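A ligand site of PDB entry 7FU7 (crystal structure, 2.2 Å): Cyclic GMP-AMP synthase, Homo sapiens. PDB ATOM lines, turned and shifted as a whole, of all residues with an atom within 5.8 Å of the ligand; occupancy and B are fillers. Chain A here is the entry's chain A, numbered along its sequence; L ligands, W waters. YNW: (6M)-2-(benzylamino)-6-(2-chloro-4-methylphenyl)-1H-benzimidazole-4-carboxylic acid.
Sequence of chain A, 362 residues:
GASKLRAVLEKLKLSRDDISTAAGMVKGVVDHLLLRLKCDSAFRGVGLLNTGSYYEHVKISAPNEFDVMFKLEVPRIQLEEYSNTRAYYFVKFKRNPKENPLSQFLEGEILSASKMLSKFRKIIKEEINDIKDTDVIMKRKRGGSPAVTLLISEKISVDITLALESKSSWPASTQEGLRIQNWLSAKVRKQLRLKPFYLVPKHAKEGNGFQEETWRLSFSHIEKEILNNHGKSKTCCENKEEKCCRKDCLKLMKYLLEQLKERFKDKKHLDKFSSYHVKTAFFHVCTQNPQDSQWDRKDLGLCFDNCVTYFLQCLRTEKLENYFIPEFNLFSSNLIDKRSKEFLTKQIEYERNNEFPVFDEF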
ATOM      1  N   GLU A  56     -21.665 -11.226  30.390  1.00  0.00           N
ATOM      2  CA  GLU A  56     -22.616 -10.321  29.745  1.00  0.00           C
ATOM      3  C   GLU A  56     -23.910 -11.093  29.619  1.00  0.00           C
ATOM      4  O   GLU A  56     -23.894 -12.282  29.311  1.00  0.00           O
ATOM      5  CB  GLU A  56     -22.110  -9.855  28.375  1.00  0.00           C
ATOM      6  CG  GLU A  56     -22.856  -8.652  27.812  1.00  0.00           C
ATOM      7  CD  GLU A  56     -23.774  -9.001  26.654  1.00  0.00           C
ATOM      8  OE1 GLU A  56     -23.432  -9.906  25.860  1.00  0.00           O
ATOM      9  OE2 GLU A  56     -24.842  -8.369  26.542  1.00  0.00           O
ATOM     10  N   VAL A  58     -26.988 -11.617  27.670  1.00  0.00           N
ATOM     11  CA  VAL A  58     -27.728 -11.434  26.427  1.00  0.00           C
ATOM     12  C   VAL A  58     -29.224 -11.573  26.650  1.00  0.00           C
ATOM     13  O   VAL A  58     -30.020 -10.733  26.189  1.00  0.00           O
ATOM     14  CB  VAL A  58     -27.232 -12.435  25.365  1.00  0.00           C
ATOM     15  CG1 VAL A  58     -28.015 -12.275  24.070  1.00  0.00           C
ATOM     16  CG2 VAL A  58     -25.742 -12.255  25.133  1.00  0.00           C
ATOM     17  N   ASP A  67     -23.172 -15.003  28.800  1.00  0.00           N
ATOM     18  CA  ASP A  67     -22.208 -14.956  27.704  1.00  0.00           C
ATOM     19  C   ASP A  67     -20.888 -14.443  28.243  1.00  0.00           C
ATOM     20  O   ASP A  67     -20.811 -13.318  28.743  1.00  0.00           O
ATOM     21  CB  ASP A  67     -22.718 -14.083  26.561  1.00  0.00           C
ATOM     22  CG  ASP A  67     -21.801 -14.116  25.348  1.00  0.00           C
ATOM     23  OD1 ASP A  67     -21.365 -15.216  24.975  1.00  0.00           O
ATOM     24  OD2 ASP A  67     -21.524 -13.041  24.781  1.00  0.00           O
ATOM     25  N   ASP A 159     -22.177 -19.212  27.601  1.00  0.00           N
ATOM     26  CA  ASP A 159     -21.463 -19.196  26.336  1.00  0.00           C
ATOM     27  C   ASP A 159     -20.082 -18.610  26.553  1.00  0.00           C
ATOM     28  O   ASP A 159     -19.957 -17.446  26.942  1.00  0.00           O
ATOM     29  CB  ASP A 159     -22.197 -18.396  25.261  1.00  0.00           C
ATOM     30  CG  ASP A 159     -23.372 -19.133  24.691  1.00  0.00           C
ATOM     31  OD1 ASP A 159     -23.593 -20.296  25.091  1.00  0.00           O
ATOM     32  OD2 ASP A 159     -24.069 -18.557  23.828  1.00  0.00           O
ATOM     33  N   LEU A 178     -18.220   4.175  14.549  1.00  0.00           N
ATOM     34  CA  LEU A 178     -18.351   4.811  15.858  1.00  0.00           C
ATOM     35  C   LEU A 178     -18.636   6.306  15.712  1.00  0.00           C
ATOM     36  O   LEU A 178     -17.946   7.159  16.272  1.00  0.00           O
ATOM     37  CB  LEU A 178     -17.106   4.557  16.707  1.00  0.00           C
ATOM     38  CG  LEU A 178     -17.152   4.818  18.209  1.00  0.00           C
ATOM     39  CD1 LEU A 178     -18.237   3.990  18.876  1.00  0.00           C
ATOM     40  CD2 LEU A 178     -15.790   4.547  18.827  1.00  0.00           C
ATOM     41  N   ARG A 216     -13.470 -12.391  12.867  1.00  0.00           N
ATOM     42  CA  ARG A 216     -14.341 -11.225  12.777  1.00  0.00           C
ATOM     43  C   ARG A 216     -13.938 -10.181  13.807  1.00  0.00           C
ATOM     44  O   ARG A 216     -13.705 -10.510  14.970  1.00  0.00           O
ATOM     45  CB  ARG A 216     -15.808 -11.610  12.982  1.00  0.00           C
ATOM     46  CG  ARG A 216     -16.772 -10.453  12.758  1.00  0.00           C
ATOM     47  CD  ARG A 216     -18.222 -10.863  12.976  1.00  0.00           C
ATOM     48  NE  ARG A 216     -18.458 -11.335  14.334  1.00  0.00           N
ATOM     49  CZ  ARG A 216     -18.653 -10.542  15.380  1.00  0.00           C
ATOM     50  NH1 ARG A 216     -18.637  -9.227  15.261  1.00  0.00           N
ATOM     51  NH2 ARG A 216     -18.879 -11.096  16.572  1.00  0.00           N
ATOM     52  N   LEU A 217     -13.829  -8.923  13.366  1.00  0.00           N
ATOM     53  CA  LEU A 217     -13.559  -7.832  14.297  1.00  0.00           C
ATOM     54  C   LEU A 217     -14.673  -7.726  15.316  1.00  0.00           C
ATOM     55  O   LEU A 217     -15.863  -7.821  14.983  1.00  0.00           O
ATOM     56  CB  LEU A 217     -13.420  -6.507  13.549  1.00  0.00           C
ATOM     57  CG  LEU A 217     -12.176  -6.295  12.700  1.00  0.00           C
ATOM     58  CD1 LEU A 217     -12.165  -4.854  12.217  1.00  0.00           C
ATOM     59  CD2 LEU A 217     -10.908  -6.622  13.478  1.00  0.00           C
ATOM     60  N   SER A 218     -14.298  -7.525  16.581  1.00  0.00           N
ATOM     61  CA  SER A 218     -15.265  -7.421  17.663  1.00  0.00           C
ATOM     62  C   SER A 218     -14.984  -6.182  18.492  1.00  0.00           C
ATOM     63  O   SER A 218     -13.823  -5.884  18.809  1.00  0.00           O
ATOM     64  CB  SER A 218     -15.234  -8.679  18.545  1.00  0.00           C
ATOM     65  OG  SER A 218     -16.429  -8.773  19.310  1.00  0.00           O
ATOM     66  N   PHE A 219     -16.043  -5.453  18.829  1.00  0.00           N
ATOM     67  CA  PHE A 219     -15.954  -4.258  19.663  1.00  0.00           C
ATOM     68  C   PHE A 219     -17.006  -4.271  20.761  1.00  0.00           C
ATOM     69  O   PHE A 219     -17.476  -3.221  21.196  1.00  0.00           O
ATOM     70  CB  PHE A 219     -16.095  -2.986  18.829  1.00  0.00           C
ATOM     71  CG  PHE A 219     -15.033  -2.820  17.782  1.00  0.00           C
ATOM     72  CD1 PHE A 219     -13.818  -2.238  18.086  1.00  0.00           C
ATOM     73  CD2 PHE A 219     -15.260  -3.244  16.477  1.00  0.00           C
ATOM     74  CE1 PHE A 219     -12.848  -2.077  17.121  1.00  0.00           C
ATOM     75  CE2 PHE A 219     -14.287  -3.097  15.512  1.00  0.00           C
ATOM     76  CZ  PHE A 219     -13.085  -2.510  15.834  1.00  0.00           C
ATOM     77  N   SER A 220     -17.387  -5.473  21.215  1.00  0.00           N
ATOM     78  CA  SER A 220     -18.447  -5.594  22.213  1.00  0.00           C
ATOM     79  C   SER A 220     -18.058  -4.966  23.546  1.00  0.00           C
ATOM     80  O   SER A 220     -18.929  -4.516  24.289  1.00  0.00           O
ATOM     81  CB  SER A 220     -18.798  -7.068  22.413  1.00  0.00           C
ATOM     82  OG  SER A 220     -17.683  -7.767  22.943  1.00  0.00           O
ATOM     83  N   HIS A 221     -16.767  -4.939  23.877  1.00  0.00           N
ATOM     84  CA  HIS A 221     -16.315  -4.334  25.119  1.00  0.00           C
ATOM     85  C   HIS A 221     -16.582  -2.831  25.173  1.00  0.00           C
ATOM     86  O   HIS A 221     -16.532  -2.244  26.252  1.00  0.00           O
ATOM     87  CB  HIS A 221     -14.825  -4.584  25.326  1.00  0.00           C
ATOM     88  CG  HIS A 221     -13.959  -4.002  24.248  1.00  0.00           C
ATOM     89  ND1 HIS A 221     -14.034  -4.404  22.937  1.00  0.00           N
ATOM     90  CD2 HIS A 221     -13.014  -3.043  24.296  1.00  0.00           C
ATOM     91  CE1 HIS A 221     -13.166  -3.725  22.214  1.00  0.00           C
ATOM     92  NE2 HIS A 221     -12.531  -2.885  23.017  1.00  0.00           N
ATOM     93  N   ILE A 222     -16.846  -2.205  24.029  1.00  0.00           N
ATOM     94  CA  ILE A 222     -17.142  -0.786  23.990  1.00  0.00           C
ATOM     95  C   ILE A 222     -18.562  -0.480  24.479  1.00  0.00           C
ATOM     96  O   ILE A 222     -18.849   0.648  24.887  1.00  0.00           O
ATOM     97  CB  ILE A 222     -16.912  -0.249  22.572  1.00  0.00           C
ATOM     98  CG1 ILE A 222     -15.491  -0.562  22.114  1.00  0.00           C
ATOM     99  CG2 ILE A 222     -17.141   1.256  22.491  1.00  0.00           C
ATOM    100  CD1 ILE A 222     -14.435   0.229  22.865  1.00  0.00           C
ATOM    101  N   GLU A 223     -19.453  -1.487  24.491  1.00  0.00           N
ATOM    102  CA  GLU A 223     -20.848  -1.233  24.850  1.00  0.00           C
ATOM    103  C   GLU A 223     -20.977  -0.771  26.294  1.00  0.00           C
ATOM    104  O   GLU A 223     -21.698   0.182  26.585  1.00  0.00           O
ATOM    105  CB  GLU A 223     -21.690  -2.486  24.604  1.00  0.00           C
ATOM    106  CG  GLU A 223     -23.183  -2.263  24.775  1.00  0.00           C
ATOM    107  CD  GLU A 223     -23.982  -3.553  24.751  1.00  0.00           C
ATOM    108  OE1 GLU A 223     -23.393  -4.610  24.445  1.00  0.00           O
ATOM    109  OE2 GLU A 223     -25.189  -3.522  25.058  1.00  0.00           O
ATOM    110  N   ILE A 226     -20.111   2.902  26.883  1.00  0.00           N
ATOM    111  CA  ILE A 226     -21.088   3.894  26.442  1.00  0.00           C
ATOM    112  C   ILE A 226     -22.377   3.817  27.248  1.00  0.00           C
ATOM    113  O   ILE A 226     -22.951   4.855  27.597  1.00  0.00           O
ATOM    114  CB  ILE A 226     -21.355   3.731  24.937  1.00  0.00           C
ATOM    115  CG1 ILE A 226     -20.079   4.007  24.150  1.00  0.00           C
ATOM    116  CG2 ILE A 226     -22.470   4.667  24.493  1.00  0.00           C
ATOM    117  CD1 ILE A 226     -20.298   4.313  22.691  1.00  0.00           C
ATOM    118  N   SER A 274     -30.379 -11.603  16.652  1.00  0.00           N
ATOM    119  CA  SER A 274     -29.940 -11.615  18.032  1.00  0.00           C
ATOM    120  C   SER A 274     -30.067 -10.213  18.614  1.00  0.00           C
ATOM    121  O   SER A 274     -30.397  -9.245  17.916  1.00  0.00           O
ATOM    122  CB  SER A 274     -28.496 -12.110  18.163  1.00  0.00           C
ATOM    123  OG  SER A 274     -27.610 -11.255  17.474  1.00  0.00           O
ATOM    124  N   SER A 275     -29.787 -10.103  19.914  1.00  0.00           N
ATOM    125  CA  SER A 275     -29.743  -8.791  20.560  1.00  0.00           C
ATOM    126  C   SER A 275     -28.698  -7.885  19.940  1.00  0.00           C
ATOM    127  O   SER A 275     -28.781  -6.657  20.091  1.00  0.00           O
ATOM    128  CB  SER A 275     -29.471  -8.959  22.058  1.00  0.00           C
ATOM    129  OG  SER A 275     -28.226  -9.572  22.283  1.00  0.00           O
ATOM    130  N   TYR A 276     -27.717  -8.452  19.235  1.00  0.00           N
ATOM    131  CA  TYR A 276     -26.688  -7.649  18.576  1.00  0.00           C
ATOM    132  C   TYR A 276     -27.292  -6.723  17.537  1.00  0.00           C
ATOM    133  O   TYR A 276     -26.956  -5.535  17.472  1.00  0.00           O
ATOM    134  CB  TYR A 276     -25.650  -8.588  17.956  1.00  0.00           C
ATOM    135  CG  TYR A 276     -24.635  -7.900  17.071  1.00  0.00           C
ATOM    136  CD1 TYR A 276     -23.877  -6.832  17.545  1.00  0.00           C
ATOM    137  CD2 TYR A 276     -24.412  -8.346  15.783  1.00  0.00           C
ATOM    138  CE1 TYR A 276     -22.939  -6.217  16.732  1.00  0.00           C
ATOM    139  CE2 TYR A 276     -23.485  -7.748  14.966  1.00  0.00           C
ATOM    140  CZ  TYR A 276     -22.751  -6.677  15.446  1.00  0.00           C
ATOM    141  OH  TYR A 276     -21.819  -6.093  14.619  1.00  0.00           O
ATOM    142  N   LYS A 279     -29.192  -4.107  19.410  1.00  0.00           N
ATOM    143  CA  LYS A 279     -28.228  -3.151  19.945  1.00  0.00           C
ATOM    144  C   LYS A 279     -27.753  -2.190  18.873  1.00  0.00           C
ATOM    145  O   LYS A 279     -27.726  -0.971  19.069  1.00  0.00           O
ATOM    146  CB  LYS A 279     -27.025  -3.864  20.555  1.00  0.00           C
ATOM    147  CG  LYS A 279     -27.244  -4.569  21.873  1.00  0.00           C
ATOM    148  CD  LYS A 279     -25.932  -5.187  22.317  1.00  0.00           C
ATOM    149  CE  LYS A 279     -26.128  -6.217  23.418  1.00  0.00           C
ATOM    150  NZ  LYS A 279     -24.847  -6.940  23.705  1.00  0.00           N
ATOM    151  N   THR A 280     -27.376  -2.738  17.706  1.00  0.00           N
ATOM    152  CA  THR A 280     -26.779  -1.934  16.652  1.00  0.00           C
ATOM    153  C   THR A 280     -27.738  -0.859  16.158  1.00  0.00           C
ATOM    154  O   THR A 280     -27.356   0.296  15.988  1.00  0.00           O
ATOM    155  CB  THR A 280     -26.352  -2.832  15.487  1.00  0.00           C
ATOM    156  OG1 THR A 280     -25.321  -3.712  15.926  1.00  0.00           O
ATOM    157  CG2 THR A 280     -25.832  -1.984  14.347  1.00  0.00           C
ATOM    158  N   PHE A 283     -28.120   2.025  18.775  1.00  0.00           N
ATOM    159  CA  PHE A 283     -27.037   3.002  18.814  1.00  0.00           C
ATOM    160  C   PHE A 283     -26.999   3.853  17.556  1.00  0.00           C
ATOM    161  O   PHE A 283     -26.507   4.991  17.595  1.00  0.00           O
ATOM    162  CB  PHE A 283     -25.698   2.291  19.034  1.00  0.00           C
ATOM    163  CG  PHE A 283     -25.492   1.832  20.450  1.00  0.00           C
ATOM    164  CD1 PHE A 283     -25.285   2.752  21.470  1.00  0.00           C
ATOM    165  CD2 PHE A 283     -25.519   0.483  20.770  1.00  0.00           C
ATOM    166  CE1 PHE A 283     -25.090   2.335  22.774  1.00  0.00           C
ATOM    167  CE2 PHE A 283     -25.330   0.058  22.072  1.00  0.00           C
ATOM    168  CZ  PHE A 283     -25.115   0.987  23.084  1.00  0.00           C
ATOM    169  N   ASN A 322     -22.990  -2.323  10.520  1.00  0.00           N
ATOM    170  CA  ASN A 322     -22.177  -2.519  11.717  1.00  0.00           C
ATOM    171  C   ASN A 322     -21.798  -1.157  12.277  1.00  0.00           C
ATOM    172  O   ASN A 322     -21.308  -0.298  11.541  1.00  0.00           O
ATOM    173  CB  ASN A 322     -20.935  -3.343  11.365  1.00  0.00           C
ATOM    174  CG  ASN A 322     -20.116  -3.719  12.585  1.00  0.00           C
ATOM    175  OD1 ASN A 322     -19.905  -2.911  13.497  1.00  0.00           O
ATOM    176  ND2 ASN A 322     -19.622  -4.949  12.607  1.00  0.00           N
ATOM    177  N   TYR A 323     -22.026  -0.964  13.571  1.00  0.00           N
ATOM    178  CA  TYR A 323     -21.840   0.360  14.167  1.00  0.00           C
ATOM    179  C   TYR A 323     -20.387   0.812  14.096  1.00  0.00           C
ATOM    180  O   TYR A 323     -20.118   2.024  14.079  1.00  0.00           O
ATOM    181  CB  TYR A 323     -22.317   0.360  15.610  1.00  0.00           C
ATOM    182  CG  TYR A 323     -22.575   1.744  16.162  1.00  0.00           C
ATOM    183  CD1 TYR A 323     -23.675   2.474  15.730  1.00  0.00           C
ATOM    184  CD2 TYR A 323     -21.721   2.314  17.102  1.00  0.00           C
ATOM    185  CE1 TYR A 323     -23.920   3.739  16.227  1.00  0.00           C
ATOM    186  CE2 TYR A 323     -21.966   3.579  17.599  1.00  0.00           C
ATOM    187  CZ  TYR A 323     -23.067   4.287  17.156  1.00  0.00           C
ATOM    188  OH  TYR A 323     -23.314   5.544  17.641  1.00  0.00           O
ATOM    189  N   PHE A 324     -19.445  -0.130  14.050  1.00  0.00           N
ATOM    190  CA  PHE A 324     -18.040   0.213  13.951  1.00  0.00           C
ATOM    191  C   PHE A 324     -17.491   0.076  12.538  1.00  0.00           C
ATOM    192  O   PHE A 324     -16.469   0.679  12.225  1.00  0.00           O
ATOM    193  CB  PHE A 324     -17.216  -0.670  14.898  1.00  0.00           C
ATOM    194  CG  PHE A 324     -17.511  -0.441  16.353  1.00  0.00           C
ATOM    195  CD1 PHE A 324     -18.670  -0.958  16.928  1.00  0.00           C
ATOM    196  CD2 PHE A 324     -16.643   0.284  17.141  1.00  0.00           C
ATOM    197  CE1 PHE A 324     -18.949  -0.740  18.262  1.00  0.00           C
ATOM    198  CE2 PHE A 324     -16.925   0.502  18.485  1.00  0.00           C
ATOM    199  CZ  PHE A 324     -18.072  -0.019  19.042  1.00  0.00           C
HETATM  200  C10 YNW L   1     -21.627   0.122  20.646  1.00  0.00           C
HETATM  201  C11 YNW L   1     -21.698   1.611  20.855  1.00  0.00           C
HETATM  202  C13 YNW L   1     -22.427  -1.884  19.598  1.00  0.00           C
HETATM  203  C15 YNW L   1     -22.238  -4.993  20.763  1.00  0.00           C
HETATM  204  C16 YNW L   1     -22.130  -6.367  20.589  1.00  0.00           C
HETATM  205  C18 YNW L   1     -22.311  -8.562  20.612  1.00  0.00           C
HETATM  206  C20 YNW L   1     -21.186  -6.954  19.741  1.00  0.00           C
HETATM  207  C22 YNW L   1     -23.847  -9.995  21.833  1.00  0.00           C
HETATM  208  C23 YNW L   1     -24.486 -11.368  21.697  1.00  0.00           C
HETATM  209  C24 YNW L   1     -25.702 -11.515  21.047  1.00  0.00           C
HETATM  210  C25 YNW L   1     -26.279 -12.761  20.922  1.00  0.00           C
HETATM  211  C26 YNW L   1     -25.650 -13.878  21.442  1.00  0.00           C
HETATM  212  C27 YNW L   1     -24.438 -13.740  22.080  1.00  0.00           C
HETATM  213  C28 YNW L   1     -23.861 -12.493  22.206  1.00  0.00           C
HETATM  214  C12 YNW L   1     -22.498  -0.524  19.779  1.00  0.00           C
HETATM  215  C2  YNW L   1     -19.285  -6.606  18.123  1.00  0.00           C
HETATM  216  C4  YNW L   1     -20.324  -6.082  19.048  1.00  0.00           C
HETATM  217  C5  YNW L   1     -20.422  -4.691  19.225  1.00  0.00           C
HETATM  218  C6  YNW L   1     -21.368  -4.141  20.080  1.00  0.00           C
HETATM  219  C7  YNW L   1     -21.473  -2.673  20.260  1.00  0.00           C
HETATM  220  C8  YNW L   1     -20.594  -2.018  21.119  1.00  0.00           C
HETATM  221  C9  YNW L   1     -20.675  -0.653  21.309  1.00  0.00           C
HETATM  222  N17 YNW L   1     -22.838  -7.431  21.131  1.00  0.00           N
HETATM  223  N19 YNW L   1     -21.324  -8.327  19.769  1.00  0.00           N
HETATM  224  N21 YNW L   1     -22.752  -9.788  20.898  1.00  0.00           N
HETATM  225  O1  YNW L   1     -18.605  -5.691  17.504  1.00  0.00           O
HETATM  226  O3  YNW L   1     -19.106  -7.801  17.974  1.00  0.00           O
HETATM  227 CL14 YNW L   1     -23.554  -2.619  18.505  1.00  0.00          CL
HETATM  228  O   HOH W   1     -21.806 -10.968  17.936  1.00  0.00           O
HETATM  229  O   HOH W   2     -20.457  -4.118  15.852  1.00  0.00           O
HETATM  230  O   HOH W   3     -17.963  -5.632  14.459  1.00  0.00           O
HETATM  231  O   HOH W   4     -22.733  -3.135  15.192  1.00  0.00           O
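N of Phe 219 is in hydrogen-bond range of O1 of the ligand.
NH1 of Arg 216 lies within salt-bridge range of O3 of the ligand (3.1 Å).
An oxygen (O3) of the ligand sits at hydrogen-bond distance from the side-chain hydroxyl (OG) of Ser 218, 3.1 Å away.
N17 of the ligand lies close to NZ of Lys 279 (3.3 Å).
OE1 of Glu 223 is in salt-bridge range of NZ of Lys 279 (2.8 Å).
NZ of Lys 279 is in salt-bridge range of OE2 of Glu 56, 3.2 Å away.
The backbone carbonyl oxygen (O) of Phe 283 lies close to the side-chain hydroxyl (OH) of Tyr 323.
The side-chain hydroxyl (OG) of Ser 274 sits close to the backbone NH (N) of Tyr 276, at 3.3 Å.
OH of Tyr 276 lies within hydrogen-bond range of ND2 of Asn 322, 3.2 Å away.
The backbone NH of Phe 324 sits at hydrogen-bond distance from the side-chain amide oxygen of Asn 322 (2.9 Å).
The backbone carbonyl oxygen (O) of Asp 67 lies within hydrogen-bond range of the backbone NH (N) of Glu 56 (2.8 Å).
The backbone NH of Leu 178 is in hydrogen-bond range of the backbone carbonyl oxygen of Tyr 323 (2.9 Å).
Val 58 touches the ligand.
OD2 of Asp 67 touches C28 of the ligand, at 3.5 Å.
CB of Ser 220 touches C20 of the ligand (3.6 Å).
C of Ile 222 touches C9 of the ligand, 3.8 Å away.
N of Glu 223 touches C9 of the ligand, 3.5 Å away.
CD1 of Ile 226 touches C11 of the ligand, 3.6 Å away.
Ser 274 touches the ligand (CB to C25, 3.6 Å).
Ser 275 touches the ligand.
Tyr 276 touches the ligand.
OG1 of Thr 280 touches CL14 of the ligand, at 3.3 Å.
Phe 283 touches the ligand.
Tyr 323 touches the ligand.
Phe 324 touches the ligand (CE1 to C9, 3.5 Å).
Of the 23 residues printed, 17 come within 4 Å of the ligand.
Water W2 lies within hydrogen-bond range of OH of Tyr 276 (2.7 Å), OD1 of Asn 322 (2.7 Å) and O1 of the ligand (2.9 Å).
Water W3 lies within hydrogen-bond range of ND2 of Asn 322 (2.6 Å), O of Leu 217 (3.1 Å) and O1 of the ligand (3.1 Å).
Water W1 bridges NH2 of Arg 216 and N19 of the ligand.
Water W4 lies within hydrogen-bond range of the side-chain hydroxyl of Thr 280, the backbone NH of Tyr 323, the side-chain hydroxyl of Tyr 276 and the side-chain amide oxygen of Asn 322.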
